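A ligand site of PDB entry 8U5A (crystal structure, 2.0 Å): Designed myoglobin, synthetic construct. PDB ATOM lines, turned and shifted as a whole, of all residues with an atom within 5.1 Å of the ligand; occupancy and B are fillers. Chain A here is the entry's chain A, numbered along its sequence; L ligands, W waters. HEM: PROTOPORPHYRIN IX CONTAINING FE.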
ATOM      1  N   PHE A  34      28.263   1.664 -31.220  1.00  0.00           N
ATOM      2  CA  PHE A  34      29.612   1.257 -31.587  1.00  0.00           C
ATOM      3  C   PHE A  34      29.905   1.506 -33.065  1.00  0.00           C
ATOM      4  O   PHE A  34      31.034   1.855 -33.419  1.00  0.00           O
ATOM      5  CB  PHE A  34      29.833  -0.213 -31.241  1.00  0.00           C
ATOM      6  CG  PHE A  34      29.800  -0.497 -29.768  1.00  0.00           C
ATOM      7  CD1 PHE A  34      30.225   0.446 -28.857  1.00  0.00           C
ATOM      8  CD2 PHE A  34      29.337  -1.717 -29.297  1.00  0.00           C
ATOM      9  CE1 PHE A  34      30.204   0.193 -27.498  1.00  0.00           C
ATOM     10  CE2 PHE A  34      29.300  -1.983 -27.945  1.00  0.00           C
ATOM     11  CZ  PHE A  34      29.734  -1.021 -27.047  1.00  0.00           C
ATOM     12  N   THR A  40      33.739   5.501 -29.096  1.00  0.00           N
ATOM     13  CA  THR A  40      33.056   5.022 -27.907  1.00  0.00           C
ATOM     14  C   THR A  40      33.357   3.544 -27.666  1.00  0.00           C
ATOM     15  O   THR A  40      33.586   3.130 -26.521  1.00  0.00           O
ATOM     16  CB  THR A  40      31.551   5.249 -28.037  1.00  0.00           C
ATOM     17  OG1 THR A  40      31.290   6.663 -28.135  1.00  0.00           O
ATOM     18  CG2 THR A  40      30.810   4.717 -26.819  1.00  0.00           C
ATOM     19  N   LEU A  41      33.378   2.745 -28.728  1.00  0.00           N
ATOM     20  CA  LEU A  41      33.719   1.329 -28.606  1.00  0.00           C
ATOM     21  C   LEU A  41      35.111   1.146 -28.029  1.00  0.00           C
ATOM     22  O   LEU A  41      35.373   0.187 -27.294  1.00  0.00           O
ATOM     23  CB  LEU A  41      33.607   0.647 -29.971  1.00  0.00           C
ATOM     24  CG  LEU A  41      34.128  -0.783 -30.070  1.00  0.00           C
ATOM     25  CD1 LEU A  41      33.308  -1.729 -29.195  1.00  0.00           C
ATOM     26  CD2 LEU A  41      34.120  -1.245 -31.520  1.00  0.00           C
ATOM     27  N   LYS A  43      36.475   2.681 -25.699  1.00  0.00           N
ATOM     28  CA  LYS A  43      36.416   2.822 -24.259  1.00  0.00           C
ATOM     29  C   LYS A  43      35.722   1.651 -23.575  1.00  0.00           C
ATOM     30  O   LYS A  43      35.560   1.674 -22.350  1.00  0.00           O
ATOM     31  CB  LYS A  43      35.718   4.132 -23.887  1.00  0.00           C
ATOM     32  CG  LYS A  43      36.304   5.348 -24.587  1.00  0.00           C
ATOM     33  CD  LYS A  43      35.845   6.631 -23.938  1.00  0.00           C
ATOM     34  CE  LYS A  43      36.274   7.840 -24.748  1.00  0.00           C
ATOM     35  NZ  LYS A  43      35.570   7.904 -26.054  1.00  0.00           N
ATOM     36  N   PHE A  44      35.301   0.642 -24.330  1.00  0.00           N
ATOM     37  CA  PHE A  44      34.705  -0.586 -23.789  1.00  0.00           C
ATOM     38  C   PHE A  44      35.655  -1.726 -24.141  1.00  0.00           C
ATOM     39  O   PHE A  44      35.527  -2.337 -25.219  1.00  0.00           O
ATOM     40  CB  PHE A  44      33.303  -0.817 -24.352  1.00  0.00           C
ATOM     41  CG  PHE A  44      32.382  -1.526 -23.409  1.00  0.00           C
ATOM     42  CD1 PHE A  44      32.799  -2.658 -22.722  1.00  0.00           C
ATOM     43  CD2 PHE A  44      31.093  -1.056 -23.192  1.00  0.00           C
ATOM     44  CE1 PHE A  44      31.950  -3.305 -21.849  1.00  0.00           C
ATOM     45  CE2 PHE A  44      30.243  -1.704 -22.319  1.00  0.00           C
ATOM     46  CZ  PHE A  44      30.667  -2.832 -21.652  1.00  0.00           C
ATOM     47  N   PRO A  45      36.615  -2.051 -23.273  1.00  0.00           N
ATOM     48  CA  PRO A  45      37.683  -2.984 -23.670  1.00  0.00           C
ATOM     49  C   PRO A  45      37.177  -4.364 -24.077  1.00  0.00           C
ATOM     50  O   PRO A  45      37.630  -4.910 -25.088  1.00  0.00           O
ATOM     51  CB  PRO A  45      38.570  -3.053 -22.415  1.00  0.00           C
ATOM     52  CG  PRO A  45      38.292  -1.784 -21.686  1.00  0.00           C
ATOM     53  CD  PRO A  45      36.843  -1.483 -21.937  1.00  0.00           C
ATOM     54  N   HIS A  65      24.522  -7.441 -22.070  1.00  0.00           N
ATOM     55  CA  HIS A  65      24.823  -6.131 -21.523  1.00  0.00           C
ATOM     56  C   HIS A  65      23.832  -5.072 -21.976  1.00  0.00           C
ATOM     57  O   HIS A  65      23.553  -4.126 -21.230  1.00  0.00           O
ATOM     58  CB  HIS A  65      26.249  -5.716 -21.892  1.00  0.00           C
ATOM     59  CG  HIS A  65      26.718  -4.488 -21.178  1.00  0.00           C
ATOM     60  ND1 HIS A  65      26.930  -4.462 -19.816  1.00  0.00           N
ATOM     61  CD2 HIS A  65      26.998  -3.251 -21.628  1.00  0.00           C
ATOM     62  CE1 HIS A  65      27.333  -3.257 -19.458  1.00  0.00           C
ATOM     63  NE2 HIS A  65      27.386  -2.502 -20.538  1.00  0.00           N
ATOM     64  N   THR A  68      21.239  -5.040 -19.536  1.00  0.00           N
ATOM     65  CA  THR A  68      21.674  -4.399 -18.299  1.00  0.00           C
ATOM     66  C   THR A  68      21.552  -2.885 -18.394  1.00  0.00           C
ATOM     67  O   THR A  68      21.107  -2.224 -17.443  1.00  0.00           O
ATOM     68  CB  THR A  68      23.117  -4.802 -17.990  1.00  0.00           C
ATOM     69  OG1 THR A  68      23.195  -6.221 -17.809  1.00  0.00           O
ATOM     70  CG2 THR A  68      23.605  -4.109 -16.721  1.00  0.00           C
ATOM     71  N   VAL A  69      21.932  -2.303 -19.532  1.00  0.00           N
ATOM     72  CA  VAL A  69      21.850  -0.861 -19.714  1.00  0.00           C
ATOM     73  C   VAL A  69      20.398  -0.405 -19.696  1.00  0.00           C
ATOM     74  O   VAL A  69      20.032   0.551 -18.996  1.00  0.00           O
ATOM     75  CB  VAL A  69      22.548  -0.437 -21.011  1.00  0.00           C
ATOM     76  CG1 VAL A  69      22.372   1.057 -21.252  1.00  0.00           C
ATOM     77  CG2 VAL A  69      24.024  -0.813 -20.977  1.00  0.00           C
ATOM     78  N   ALA A  72      18.686  -0.430 -16.274  1.00  0.00           N
ATOM     79  CA  ALA A  72      19.017   0.702 -15.422  1.00  0.00           C
ATOM     80  C   ALA A  72      18.209   1.932 -15.801  1.00  0.00           C
ATOM     81  O   ALA A  72      17.689   2.635 -14.919  1.00  0.00           O
ATOM     82  CB  ALA A  72      20.511   1.002 -15.515  1.00  0.00           C
ATOM     83  N   LEU A  73      18.071   2.209 -17.101  1.00  0.00           N
ATOM     84  CA  LEU A  73      17.282   3.352 -17.534  1.00  0.00           C
ATOM     85  C   LEU A  73      15.807   3.173 -17.191  1.00  0.00           C
ATOM     86  O   LEU A  73      15.154   4.124 -16.733  1.00  0.00           O
ATOM     87  CB  LEU A  73      17.452   3.561 -19.040  1.00  0.00           C
ATOM     88  CG  LEU A  73      18.803   4.077 -19.533  1.00  0.00           C
ATOM     89  CD1 LEU A  73      18.907   3.929 -21.046  1.00  0.00           C
ATOM     90  CD2 LEU A  73      19.012   5.526 -19.121  1.00  0.00           C
ATOM     91  N   GLU A  92      25.578   5.757  -7.778  1.00  0.00           N
ATOM     92  CA  GLU A  92      26.462   4.611  -8.004  1.00  0.00           C
ATOM     93  C   GLU A  92      26.653   4.329  -9.492  1.00  0.00           C
ATOM     94  O   GLU A  92      27.681   3.764  -9.876  1.00  0.00           O
ATOM     95  CB  GLU A  92      25.917   3.377  -7.275  1.00  0.00           C
ATOM     96  CG  GLU A  92      24.527   2.949  -7.692  1.00  0.00           C
ATOM     97  CD  GLU A  92      23.886   2.001  -6.678  1.00  0.00           C
ATOM     98  OE1 GLU A  92      24.115   2.183  -5.471  1.00  0.00           O
ATOM     99  OE2 GLU A  92      23.165   1.070  -7.108  1.00  0.00           O
ATOM    100  N   LEU A  93      25.697   4.720 -10.336  1.00  0.00           N
ATOM    101  CA  LEU A  93      25.893   4.579 -11.775  1.00  0.00           C
ATOM    102  C   LEU A  93      26.909   5.593 -12.276  1.00  0.00           C
ATOM    103  O   LEU A  93      27.737   5.274 -13.139  1.00  0.00           O
ATOM    104  CB  LEU A  93      24.561   4.739 -12.505  1.00  0.00           C
ATOM    105  CG  LEU A  93      24.512   4.247 -13.950  1.00  0.00           C
ATOM    106  CD1 LEU A  93      24.823   2.754 -14.010  1.00  0.00           C
ATOM    107  CD2 LEU A  93      23.162   4.533 -14.588  1.00  0.00           C
ATOM    108  N   SER A  96      30.568   4.572 -10.865  1.00  0.00           N
ATOM    109  CA  SER A  96      31.211   3.471 -11.562  1.00  0.00           C
ATOM    110  C   SER A  96      31.709   3.883 -12.946  1.00  0.00           C
ATOM    111  O   SER A  96      32.690   3.329 -13.438  1.00  0.00           O
ATOM    112  CB  SER A  96      30.251   2.291 -11.675  1.00  0.00           C
ATOM    113  OG  SER A  96      29.077   2.664 -12.382  1.00  0.00           O
ATOM    114  N   HIS A  97      31.037   4.845 -13.583  1.00  0.00           N
ATOM    115  CA  HIS A  97      31.395   5.231 -14.945  1.00  0.00           C
ATOM    116  C   HIS A  97      32.398   6.375 -14.993  1.00  0.00           C
ATOM    117  O   HIS A  97      33.100   6.516 -15.996  1.00  0.00           O
ATOM    118  CB  HIS A  97      30.135   5.590 -15.726  1.00  0.00           C
ATOM    119  CG  HIS A  97      29.242   4.428 -15.995  1.00  0.00           C
ATOM    120  ND1 HIS A  97      28.528   3.784 -15.001  1.00  0.00           N
ATOM    121  CD2 HIS A  97      28.944   3.767 -17.138  1.00  0.00           C
ATOM    122  CE1 HIS A  97      27.837   2.797 -15.519  1.00  0.00           C
ATOM    123  NE2 HIS A  97      28.072   2.763 -16.818  1.00  0.00           N
ATOM    124  N   HIS A 101      34.975   2.863 -14.787  1.00  0.00           N
ATOM    125  CA  HIS A 101      34.989   2.664 -16.229  1.00  0.00           C
ATOM    126  C   HIS A 101      35.646   3.806 -16.989  1.00  0.00           C
ATOM    127  O   HIS A 101      36.119   3.592 -18.108  1.00  0.00           O
ATOM    128  CB  HIS A 101      33.566   2.469 -16.753  1.00  0.00           C
ATOM    129  CG  HIS A 101      32.785   1.448 -15.996  1.00  0.00           C
ATOM    130  ND1 HIS A 101      33.351   0.280 -15.516  1.00  0.00           N
ATOM    131  CD2 HIS A 101      31.486   1.410 -15.606  1.00  0.00           C
ATOM    132  CE1 HIS A 101      32.442  -0.430 -14.886  1.00  0.00           C
ATOM    133  NE2 HIS A 101      31.293   0.231 -14.924  1.00  0.00           N
ATOM    134  N   ILE A 103      34.417   6.798 -18.317  1.00  0.00           N
ATOM    135  CA  ILE A 103      33.646   7.076 -19.526  1.00  0.00           C
ATOM    136  C   ILE A 103      33.235   8.546 -19.507  1.00  0.00           C
ATOM    137  O   ILE A 103      32.558   8.976 -18.573  1.00  0.00           O
ATOM    138  CB  ILE A 103      32.420   6.161 -19.642  1.00  0.00           C
ATOM    139  CG1 ILE A 103      32.831   4.696 -19.540  1.00  0.00           C
ATOM    140  CG2 ILE A 103      31.709   6.405 -20.963  1.00  0.00           C
ATOM    141  CD1 ILE A 103      33.880   4.285 -20.551  1.00  0.00           C
ATOM    142  N   ASP A 107      30.102  10.218 -24.273  1.00  0.00           N
ATOM    143  CA  ASP A 107      29.868   8.837 -24.689  1.00  0.00           C
ATOM    144  C   ASP A 107      28.540   8.313 -24.157  1.00  0.00           C
ATOM    145  O   ASP A 107      27.873   7.524 -24.833  1.00  0.00           O
ATOM    146  CB  ASP A 107      31.024   7.948 -24.220  1.00  0.00           C
ATOM    147  CG  ASP A 107      32.316   8.228 -24.961  1.00  0.00           C
ATOM    148  OD1 ASP A 107      32.396   7.925 -26.169  1.00  0.00           O
ATOM    149  OD2 ASP A 107      33.247   8.763 -24.332  1.00  0.00           O
ATOM    150  N   LEU A 108      28.151   8.751 -22.960  1.00  0.00           N
ATOM    151  CA  LEU A 108      26.830   8.405 -22.443  1.00  0.00           C
ATOM    152  C   LEU A 108      25.728   8.974 -23.332  1.00  0.00           C
ATOM    153  O   LEU A 108      24.699   8.320 -23.543  1.00  0.00           O
ATOM    154  CB  LEU A 108      26.676   8.935 -21.008  1.00  0.00           C
ATOM    155  CG  LEU A 108      27.054   8.025 -19.843  1.00  0.00           C
ATOM    156  CD1 LEU A 108      28.388   7.341 -20.046  1.00  0.00           C
ATOM    157  CD2 LEU A 108      27.078   8.851 -18.564  1.00  0.00           C
ATOM    158  N   ILE A 111      24.900   6.706 -26.291  1.00  0.00           N
ATOM    159  CA  ILE A 111      23.964   5.632 -25.991  1.00  0.00           C
ATOM    160  C   ILE A 111      22.538   6.141 -26.049  1.00  0.00           C
ATOM    161  O   ILE A 111      21.658   5.520 -26.665  1.00  0.00           O
ATOM    162  CB  ILE A 111      24.291   5.000 -24.624  1.00  0.00           C
ATOM    163  CG1 ILE A 111      25.667   4.341 -24.641  1.00  0.00           C
ATOM    164  CG2 ILE A 111      23.219   3.978 -24.229  1.00  0.00           C
ATOM    165  CD1 ILE A 111      25.723   3.058 -25.445  1.00  0.00           C
ATOM    166  N   ALA A 112      22.278   7.284 -25.411  1.00  0.00           N
ATOM    167  CA  ALA A 112      20.922   7.846 -25.398  1.00  0.00           C
ATOM    168  C   ALA A 112      20.473   8.227 -26.807  1.00  0.00           C
ATOM    169  O   ALA A 112      19.312   8.042 -27.158  1.00  0.00           O
ATOM    170  CB  ALA A 112      20.869   9.061 -24.467  1.00  0.00           C
ATOM    171  N   PHE A 142      18.354  12.546 -17.647  1.00  0.00           N
ATOM    172  CA  PHE A 142      19.231  11.507 -17.098  1.00  0.00           C
ATOM    173  C   PHE A 142      20.698  11.884 -17.265  1.00  0.00           C
ATOM    174  O   PHE A 142      21.502  11.719 -16.329  1.00  0.00           O
ATOM    175  CB  PHE A 142      18.933  10.170 -17.774  1.00  0.00           C
ATOM    176  CG  PHE A 142      20.002   9.135 -17.559  1.00  0.00           C
ATOM    177  CD1 PHE A 142      20.099   8.468 -16.355  1.00  0.00           C
ATOM    178  CD2 PHE A 142      20.895   8.821 -18.568  1.00  0.00           C
ATOM    179  CE1 PHE A 142      21.086   7.510 -16.151  1.00  0.00           C
ATOM    180  CE2 PHE A 142      21.875   7.871 -18.374  1.00  0.00           C
ATOM    181  CZ  PHE A 142      21.975   7.218 -17.161  1.00  0.00           C
ATOM    182  N   ILE A 143      21.062  12.379 -18.445  1.00  0.00           N
ATOM    183  CA  ILE A 143      22.458  12.752 -18.698  1.00  0.00           C
ATOM    184  C   ILE A 143      22.874  13.898 -17.783  1.00  0.00           C
ATOM    185  O   ILE A 143      23.986  13.895 -17.222  1.00  0.00           O
ATOM    186  CB  ILE A 143      22.651  13.088 -20.186  1.00  0.00           C
ATOM    187  CG1 ILE A 143      22.438  11.843 -21.036  1.00  0.00           C
ATOM    188  CG2 ILE A 143      24.026  13.679 -20.445  1.00  0.00           C
ATOM    189  CD1 ILE A 143      23.435  10.747 -20.761  1.00  0.00           C
HETATM  190  CHA HEM L   1      28.530  -1.389 -16.843  1.00  0.00           C
HETATM  191  CHB HEM L   1      24.618   1.423 -17.598  1.00  0.00           C
HETATM  192  CHC HEM L   1      27.099   3.996 -20.896  1.00  0.00           C
HETATM  193  CHD HEM L   1      31.017   1.241 -20.065  1.00  0.00           C
HETATM  194  C1A HEM L   1      27.261  -0.846 -16.733  1.00  0.00           C
HETATM  195  C2A HEM L   1      26.216  -1.263 -15.806  1.00  0.00           C
HETATM  196  C3A HEM L   1      25.148  -0.487 -16.020  1.00  0.00           C
HETATM  197  C4A HEM L   1      25.454   0.452 -17.082  1.00  0.00           C
HETATM  198  CMA HEM L   1      23.795  -0.577 -15.270  1.00  0.00           C
HETATM  199  CAA HEM L   1      26.326  -2.408 -14.775  1.00  0.00           C
HETATM  200  CBA HEM L   1      26.528  -1.844 -13.366  1.00  0.00           C
HETATM  201  CGA HEM L   1      27.655  -0.842 -13.341  1.00  0.00           C
HETATM  202  O1A HEM L   1      27.423   0.302 -12.866  1.00  0.00           O
HETATM  203  O2A HEM L   1      28.773  -1.184 -13.799  1.00  0.00           O
HETATM  204  C1B HEM L   1      24.932   2.371 -18.551  1.00  0.00           C
HETATM  205  C2B HEM L   1      24.059   3.426 -19.062  1.00  0.00           C
HETATM  206  C3B HEM L   1      24.760   4.138 -19.970  1.00  0.00           C
HETATM  207  C4B HEM L   1      26.080   3.559 -20.070  1.00  0.00           C
HETATM  208  CMB HEM L   1      22.603   3.624 -18.580  1.00  0.00           C
HETATM  209  CAB HEM L   1      24.327   5.364 -20.835  1.00  0.00           C
HETATM  210  CBB HEM L   1      23.112   5.917 -20.830  1.00  0.00           C
HETATM  211  C1C HEM L   1      28.341   3.396 -21.050  1.00  0.00           C
HETATM  212  C2C HEM L   1      29.269   3.586 -22.152  1.00  0.00           C
HETATM  213  C3C HEM L   1      30.349   2.832 -21.910  1.00  0.00           C
HETATM  214  C4C HEM L   1      30.133   2.125 -20.662  1.00  0.00           C
HETATM  215  CMC HEM L   1      28.996   4.534 -23.337  1.00  0.00           C
HETATM  216  CAC HEM L   1      31.650   2.635 -22.744  1.00  0.00           C
HETATM  217  CBC HEM L   1      31.853   3.123 -23.963  1.00  0.00           C
HETATM  218  C1D HEM L   1      30.695   0.261 -19.160  1.00  0.00           C
HETATM  219  C2D HEM L   1      31.544  -0.826 -18.726  1.00  0.00           C
HETATM  220  C3D HEM L   1      30.848  -1.547 -17.837  1.00  0.00           C
HETATM  221  C4D HEM L   1      29.535  -0.949 -17.669  1.00  0.00           C
HETATM  222  CMD HEM L   1      32.986  -1.120 -19.189  1.00  0.00           C
HETATM  223  CAD HEM L   1      31.367  -2.815 -17.115  1.00  0.00           C
HETATM  224  CBD HEM L   1      30.710  -4.039 -17.736  1.00  0.00           C
HETATM  225  CGD HEM L   1      31.353  -5.284 -17.175  1.00  0.00           C
HETATM  226  O1D HEM L   1      32.334  -5.153 -16.395  1.00  0.00           O
HETATM  227  O2D HEM L   1      30.900  -6.402 -17.527  1.00  0.00           O
HETATM  228  NA  HEM L   1      26.755   0.207 -17.499  1.00  0.00           N
HETATM  229  NB  HEM L   1      26.158   2.483 -19.193  1.00  0.00           N
HETATM  230  NC  HEM L   1      28.900   2.496 -20.169  1.00  0.00           N
HETATM  231  ND  HEM L   1      29.479   0.156 -18.499  1.00  0.00           N
HETATM  232 FE   HEM L   1      27.802   1.274 -18.942  1.00  0.00          FE
HETATM  233  O   HOH W   1      33.635  -5.697 -19.443  1.00  0.00           O
HETATM  234  O   HOH W   2      27.303   0.067 -20.581  1.00  0.00           O
HETATM  235  O   HOH W   3      30.318  -6.970 -20.429  1.00  0.00           O
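OD2 of Asp 107 lies within salt-bridge range of NZ of Lys 43.
The backbone carbonyl oxygen (O) of His 97 is in hydrogen-bond range of the backbone NH (N) of Ile 103 (2.7 Å).
OG of Ser 96 is in hydrogen-bond range of O of Leu 93, 3.0 Å away.
The side-chain hydroxyl (OG) of Ser 96 lies within hydrogen-bond range of the backbone carbonyl oxygen (O) of Glu 92, 3.1 Å away.
OD1 of Asp 107 is in hydrogen-bond range of OG1 of Thr 40, 2.6 Å away.
A ring nitrogen (ND1) of His 97 sits at hydrogen-bond distance from the backbone carbonyl oxygen (O) of Leu 93.
The backbone NH (N) of His 101 is in hydrogen-bond range of the backbone carbonyl oxygen (O) of Ser 96.
ND1 of His 97 sits at hydrogen-bond distance from OG of Ser 96 (2.9 Å).
NA of the ligand sits close to NE2 of His 97 (3.0 Å).
Thr 40 touches the ligand.
Lys 43 touches the ligand (CB to CBC, 3.995 Å).
CE1 of Phe 44 touches CMD of the ligand, 3.6 Å away.
His 65 touches the ligand.
Thr 68 touches the ligand.
Val 69 touches the ligand.
CB of Ala 72 touches CMA of the ligand, at 3.7 Å.
Leu 73 touches the ligand.
CD1 of Leu 93 touches CMA of the ligand, 3.7 Å away.
Ile 103 touches the ligand (CD1 to CAC, 3.5 Å).
Asp 107 touches the ligand.
Leu 108 touches the ligand (CD1 to CHC, 3.7 Å).
Ile 111 touches the ligand.
Phe 142 touches the ligand.
The nearest printed residue that does not touch the ligand is Glu 92 (4.6 Å).
An oxygen (O2A) of the ligand is in hydrogen-bond range of a ring nitrogen (NE2) of His 101, at 3.1 Å.
The side-chain hydroxyl of Ser 96 sits at hydrogen-bond distance from an oxygen (O1A) of the ligand.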
